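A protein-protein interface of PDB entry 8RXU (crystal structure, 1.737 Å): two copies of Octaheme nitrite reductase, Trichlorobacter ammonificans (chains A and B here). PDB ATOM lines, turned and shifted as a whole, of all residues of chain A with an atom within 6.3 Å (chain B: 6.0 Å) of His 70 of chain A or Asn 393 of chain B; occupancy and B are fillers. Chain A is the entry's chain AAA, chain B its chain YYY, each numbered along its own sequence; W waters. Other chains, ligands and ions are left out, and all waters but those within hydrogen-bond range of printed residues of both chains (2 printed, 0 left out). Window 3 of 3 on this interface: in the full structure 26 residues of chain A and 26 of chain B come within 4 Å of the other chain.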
ATOM      1  N   VAL A  68     -11.075 -10.466 -21.034  1.00  0.00           N
ATOM      2  CA  VAL A  68     -12.409 -10.525 -21.698  1.00  0.00           C
ATOM      3  C   VAL A  68     -13.040  -9.143 -21.564  1.00  0.00           C
ATOM      4  O   VAL A  68     -13.031  -8.572 -20.449  1.00  0.00           O
ATOM      5  CB  VAL A  68     -13.355 -11.563 -21.053  1.00  0.00           C
ATOM      6  CG1 VAL A  68     -14.777 -11.382 -21.539  1.00  0.00           C
ATOM      7  CG2 VAL A  68     -12.928 -13.000 -21.258  1.00  0.00           C
ATOM      8  N   HIS A  69     -13.578  -8.627 -22.658  1.00  0.00           N
ATOM      9  CA  HIS A  69     -14.393  -7.402 -22.681  1.00  0.00           C
ATOM     10  C   HIS A  69     -15.555  -7.668 -23.611  1.00  0.00           C
ATOM     11  O   HIS A  69     -15.308  -8.314 -24.622  1.00  0.00           O
ATOM     12  CB  HIS A  69     -13.632  -6.185 -23.180  1.00  0.00           C
ATOM     13  CG  HIS A  69     -12.560  -5.797 -22.237  1.00  0.00           C
ATOM     14  ND1 HIS A  69     -12.791  -5.751 -20.884  1.00  0.00           N
ATOM     15  CD2 HIS A  69     -11.258  -5.502 -22.444  1.00  0.00           C
ATOM     16  CE1 HIS A  69     -11.670  -5.389 -20.281  1.00  0.00           C
ATOM     17  NE2 HIS A  69     -10.721  -5.211 -21.225  1.00  0.00           N
ATOM     18  N   HIS A  70     -16.735  -7.198 -23.242  1.00  0.00           N
ATOM     19  CA  HIS A  70     -17.947  -7.276 -24.086  1.00  0.00           C
ATOM     20  C   HIS A  70     -18.462  -5.900 -24.422  1.00  0.00           C
ATOM     21  O   HIS A  70     -19.011  -5.203 -23.569  1.00  0.00           O
ATOM     22  CB  HIS A  70     -18.998  -8.145 -23.413  1.00  0.00           C
ATOM     23  CG  HIS A  70     -18.487  -9.518 -23.322  1.00  0.00           C
ATOM     24  ND1 HIS A  70     -18.032 -10.033 -22.134  1.00  0.00           N
ATOM     25  CD2 HIS A  70     -18.281 -10.456 -24.271  1.00  0.00           C
ATOM     26  CE1 HIS A  70     -17.661 -11.268 -22.325  1.00  0.00           C
ATOM     27  NE2 HIS A  70     -17.791 -11.545 -23.634  1.00  0.00           N
ATOM     28  N   ASP A  71     -18.291  -5.527 -25.680  1.00  0.00           N
ATOM     29  CA  ASP A  71     -18.958  -4.329 -26.233  1.00  0.00           C
ATOM     30  C   ASP A  71     -20.446  -4.620 -26.420  1.00  0.00           C
ATOM     31  O   ASP A  71     -20.800  -5.605 -27.086  1.00  0.00           O
ATOM     32  CB  ASP A  71     -18.346  -3.914 -27.564  1.00  0.00           C
ATOM     33  CG  ASP A  71     -18.868  -2.565 -28.030  1.00  0.00           C
ATOM     34  OD1 ASP A  71     -20.065  -2.215 -27.790  1.00  0.00           O
ATOM     35  OD2 ASP A  71     -18.087  -1.864 -28.654  1.00  0.00           O
ATOM     36  N   PRO A  72     -21.360  -3.832 -25.804  1.00  0.00           N
ATOM     37  CA  PRO A  72     -22.811  -4.067 -25.888  1.00  0.00           C
ATOM     38  C   PRO A  72     -23.441  -3.879 -27.281  1.00  0.00           C
ATOM     39  O   PRO A  72     -24.571  -4.318 -27.460  1.00  0.00           O
ATOM     40  CB  PRO A  72     -23.441  -3.031 -24.942  1.00  0.00           C
ATOM     41  CG  PRO A  72     -22.374  -2.002 -24.716  1.00  0.00           C
ATOM     42  CD  PRO A  72     -21.081  -2.783 -24.807  1.00  0.00           C
ATOM     43  N   THR A  73     -22.657  -3.309 -28.197  1.00  0.00           N
ATOM     44  CA  THR A  73     -22.953  -3.109 -29.642  1.00  0.00           C
ATOM     45  C   THR A  73     -22.435  -4.324 -30.425  1.00  0.00           C
ATOM     46  O   THR A  73     -22.473  -4.311 -31.650  1.00  0.00           O
ATOM     47  CB  THR A  73     -22.383  -1.760 -30.106  1.00  0.00           C
ATOM     48  OG1 THR A  73     -20.949  -1.702 -30.121  1.00  0.00           O
ATOM     49  CG2 THR A  73     -22.883  -0.609 -29.254  1.00  0.00           C
ATOM     50  N   TYR A 110      -8.101 -11.479 -30.303  1.00  0.00           N
ATOM     51  CA  TYR A 110      -8.985 -12.077 -31.359  1.00  0.00           C
ATOM     52  C   TYR A 110      -8.339 -12.116 -32.743  1.00  0.00           C
ATOM     53  O   TYR A 110      -8.981 -12.557 -33.692  1.00  0.00           O
ATOM     54  CB  TYR A 110     -10.364 -11.390 -31.425  1.00  0.00           C
ATOM     55  CG  TYR A 110     -11.098 -11.552 -30.127  1.00  0.00           C
ATOM     56  CD1 TYR A 110     -11.557 -12.798 -29.708  1.00  0.00           C
ATOM     57  CD2 TYR A 110     -11.195 -10.488 -29.262  1.00  0.00           C
ATOM     58  CE1 TYR A 110     -12.147 -12.949 -28.474  1.00  0.00           C
ATOM     59  CE2 TYR A 110     -11.723 -10.642 -27.995  1.00  0.00           C
ATOM     60  CZ  TYR A 110     -12.206 -11.870 -27.610  1.00  0.00           C
ATOM     61  OH  TYR A 110     -12.831 -11.966 -26.409  1.00  0.00           O
ATOM     62  N   ASP A 136     -16.502 -14.810 -28.083  1.00  0.00           N
ATOM     63  CA  ASP A 136     -15.692 -13.960 -27.164  1.00  0.00           C
ATOM     64  C   ASP A 136     -14.536 -14.749 -26.524  1.00  0.00           C
ATOM     65  O   ASP A 136     -13.953 -14.235 -25.588  1.00  0.00           O
ATOM     66  CB  ASP A 136     -16.614 -13.419 -26.081  1.00  0.00           C
ATOM     67  CG  ASP A 136     -17.125 -14.531 -25.179  1.00  0.00           C
ATOM     68  OD1 ASP A 136     -17.284 -15.687 -25.689  1.00  0.00           O
ATOM     69  OD2 ASP A 136     -17.376 -14.248 -24.009  1.00  0.00           O
ATOM     70  N   VAL B 379     -31.761  -7.943 -20.440  1.00  0.00           N
ATOM     71  CA  VAL B 379     -30.830  -9.095 -20.599  1.00  0.00           C
ATOM     72  C   VAL B 379     -30.800  -9.886 -19.278  1.00  0.00           C
ATOM     73  O   VAL B 379     -30.640 -11.133 -19.327  1.00  0.00           O
ATOM     74  CB  VAL B 379     -29.435  -8.712 -21.153  1.00  0.00           C
ATOM     75  CG1 VAL B 379     -29.566  -8.150 -22.574  1.00  0.00           C
ATOM     76  CG2 VAL B 379     -28.645  -7.700 -20.343  1.00  0.00           C
ATOM     77  N   THR B 391     -22.589 -11.554 -18.034  1.00  0.00           N
ATOM     78  CA  THR B 391     -22.767 -10.150 -17.610  1.00  0.00           C
ATOM     79  C   THR B 391     -23.768  -9.481 -18.555  1.00  0.00           C
ATOM     80  O   THR B 391     -23.920  -9.917 -19.712  1.00  0.00           O
ATOM     81  CB  THR B 391     -21.450  -9.375 -17.629  1.00  0.00           C
ATOM     82  OG1 THR B 391     -21.082  -9.271 -19.009  1.00  0.00           O
ATOM     83  CG2 THR B 391     -20.357 -10.025 -16.805  1.00  0.00           C
ATOM     84  N   PRO B 392     -24.464  -8.401 -18.134  1.00  0.00           N
ATOM     85  CA  PRO B 392     -25.365  -7.693 -19.043  1.00  0.00           C
ATOM     86  C   PRO B 392     -24.617  -7.364 -20.353  1.00  0.00           C
ATOM     87  O   PRO B 392     -25.136  -7.648 -21.380  1.00  0.00           O
ATOM     88  CB  PRO B 392     -25.780  -6.433 -18.274  1.00  0.00           C
ATOM     89  CG  PRO B 392     -25.651  -6.842 -16.811  1.00  0.00           C
ATOM     90  CD  PRO B 392     -24.508  -7.840 -16.768  1.00  0.00           C
ATOM     91  N   ASN B 393     -23.377  -6.895 -20.264  1.00  0.00           N
ATOM     92  CA  ASN B 393     -22.585  -6.540 -21.486  1.00  0.00           C
ATOM     93  C   ASN B 393     -22.447  -7.755 -22.409  1.00  0.00           C
ATOM     94  O   ASN B 393     -22.673  -7.613 -23.638  1.00  0.00           O
ATOM     95  CB  ASN B 393     -21.219  -6.002 -21.140  1.00  0.00           C
ATOM     96  CG  ASN B 393     -21.270  -4.537 -20.789  1.00  0.00           C
ATOM     97  OD1 ASN B 393     -22.187  -3.808 -21.180  1.00  0.00           O
ATOM     98  ND2 ASN B 393     -20.256  -4.102 -20.057  1.00  0.00           N
ATOM     99  N   LYS B 394     -22.066  -8.897 -21.862  1.00  0.00           N
ATOM    100  CA  LYS B 394     -21.826 -10.131 -22.642  1.00  0.00           C
ATOM    101  C   LYS B 394     -23.117 -10.508 -23.364  1.00  0.00           C
ATOM    102  O   LYS B 394     -23.008 -10.851 -24.571  1.00  0.00           O
ATOM    103  CB  LYS B 394     -21.333 -11.299 -21.786  1.00  0.00           C
ATOM    104  CG  LYS B 394     -21.329 -12.619 -22.552  1.00  0.00           C
ATOM    105  CD  LYS B 394     -20.148 -13.466 -22.261  1.00  0.00           C
ATOM    106  CE  LYS B 394     -20.279 -14.905 -22.658  1.00  0.00           C
ATOM    107  NZ  LYS B 394     -19.007 -15.655 -22.529  1.00  0.00           N
ATOM    108  N   ALA B 395     -24.261 -10.489 -22.662  1.00  0.00           N
ATOM    109  CA  ALA B 395     -25.618 -10.801 -23.211  1.00  0.00           C
ATOM    110  C   ALA B 395     -25.879  -9.901 -24.396  1.00  0.00           C
ATOM    111  O   ALA B 395     -26.211 -10.359 -25.517  1.00  0.00           O
ATOM    112  CB  ALA B 395     -26.699 -10.578 -22.186  1.00  0.00           C
ATOM    113  N   LYS B 396     -25.733  -8.613 -24.165  1.00  0.00           N
ATOM    114  CA  LYS B 396     -25.926  -7.615 -25.225  1.00  0.00           C
ATOM    115  C   LYS B 396     -24.951  -7.910 -26.370  1.00  0.00           C
ATOM    116  O   LYS B 396     -25.362  -7.775 -27.581  1.00  0.00           O
ATOM    117  CB  LYS B 396     -25.730  -6.259 -24.579  1.00  0.00           C
ATOM    118  CG  LYS B 396     -26.906  -5.752 -23.777  1.00  0.00           C
ATOM    119  CD  LYS B 396     -26.467  -4.680 -22.771  1.00  0.00           C
ATOM    120  CE  LYS B 396     -27.571  -3.803 -22.250  1.00  0.00           C
ATOM    121  NZ  LYS B 396     -27.077  -2.967 -21.126  1.00  0.00           N
ATOM    122  N   PHE B 397     -23.684  -8.181 -26.020  1.00  0.00           N
ATOM    123  CA  PHE B 397     -22.618  -8.465 -26.998  1.00  0.00           C
ATOM    124  C   PHE B 397     -23.146  -9.598 -27.866  1.00  0.00           C
ATOM    125  O   PHE B 397     -23.083  -9.522 -29.113  1.00  0.00           O
ATOM    126  CB  PHE B 397     -21.315  -8.831 -26.306  1.00  0.00           C
ATOM    127  CG  PHE B 397     -20.255  -9.373 -27.214  1.00  0.00           C
ATOM    128  CD1 PHE B 397     -19.387  -8.511 -27.869  1.00  0.00           C
ATOM    129  CD2 PHE B 397     -20.161 -10.730 -27.471  1.00  0.00           C
ATOM    130  CE1 PHE B 397     -18.379  -9.008 -28.683  1.00  0.00           C
ATOM    131  CE2 PHE B 397     -19.134 -11.222 -28.260  1.00  0.00           C
ATOM    132  CZ  PHE B 397     -18.263 -10.354 -28.893  1.00  0.00           C
ATOM    133  N   MET B 398     -23.648 -10.665 -27.251  1.00  0.00           N
ATOM    134  CA  MET B 398     -24.064 -11.842 -28.073  1.00  0.00           C
ATOM    135  C   MET B 398     -25.196 -11.470 -29.036  1.00  0.00           C
ATOM    136  O   MET B 398     -25.011 -11.735 -30.246  1.00  0.00           O
ATOM    137  CB  MET B 398     -24.444 -13.047 -27.211  1.00  0.00           C
ATOM    138  CG  MET B 398     -23.211 -13.727 -26.626  1.00  0.00           C
ATOM    139  SD  MET B 398     -21.971 -14.309 -27.804  1.00  0.00           S
ATOM    140  CE  MET B 398     -20.942 -15.233 -26.667  1.00  0.00           C
HETATM  141  O   HOH W   1     -18.422 -17.523 -24.564  1.00  0.00           O
HETATM  142  O   HOH W   2     -18.359  -8.778 -19.525  1.00  0.00           O
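OD2 of Asp 136 of chain A is in salt-bridge range of NZ of Lys 394 of chain B (2.6 Å).
The side-chain carboxylate of Asp 71 of chain A is in hydrogen-bond range of the side-chain hydroxyl of Thr 73 of chain A (2.5 Å). OG1 of Thr 391 of chain B sits at hydrogen-bond distance from N of Lys 394 of chain B, at 3.0 Å. O of Asp 136 of chain A lies within hydrogen-bond range of OH of Tyr 110 of chain A. A ring nitrogen (NE2) of His 70 of chain A sits at hydrogen-bond distance from the side-chain carboxylate (OD2) of Asp 136 of chain A (2.8 Å).
His 70 of chain A touches Asn 393 of chain B (O to CB, 3.4 Å). His 70 of chain A touches Lys 394 of chain B. Phe 397 of chain B touches His 70 of chain A. O of Asp 71 of chain A touches CD1 of Phe 397 of chain B, at 3.3 Å. CD of Pro 72 of chain A touches OD1 of Asn 393 of chain B, at 3.9 Å. Lys 396 of chain B touches Pro 72 of chain A (O to O, 3.5 Å). CB of Asp 136 of chain A touches CE2 of Phe 397 of chain B, at 3.99 Å. CE of Met 398 of chain B touches OD1 of Asp 136 of chain A, at 3.8 Å.
Of chain B, only Asn 393 (3.4 Å), Lys 394 (3.3 Å) and Phe 397 (3.7 Å) come within 4 Å of His 70 of chain A. Printed residues of chain B within 4 Å of Pro 72 of chain A: Asn 393 and Lys 396. Printed residues of chain B within 4 Å of Asp 136 of chain A: Lys 394 (2.6 Å), Phe 397 (3.99 Å) and Met 398 (3.8 Å). Asn 393 of chain B touches just these residues of chain A: His 70 (3.4 Å) and Pro 72 (3.9 Å). The nearest residue of chain A that does not touch Asn 393 of chain B is Asp 71 of chain A (4.4 Å).
Of the 8 printed residues of chain A, 4 touch a printed residue of chain B. Printed residues of chain A that touch a printed residue of chain B: His 70, Asp 71, Pro 72 and Asp 136. Hydrophobic or aromatic side chains of chain B that line the printed part of chain A: Phe 397 and Met 398. Among the printed residues, 9 pairs touch across the chains. Among the printed residues, Asp or Glu carboxylates within 4 Å of a Lys or Arg side-chain nitrogen of the other chain: Asp 136 of chain A with Lys 394 of chain B.
No position is printed for both chains.
Water W1 bridges OD1 of Asp 136 of chain A (2.4 Å) and NZ of Lys 394 of chain B (2.8 Å). Water W2 bridges OG1 of Thr 391 of chain B (2.8 Å) and ND1 of His 70 of chain A (2.9 Å).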
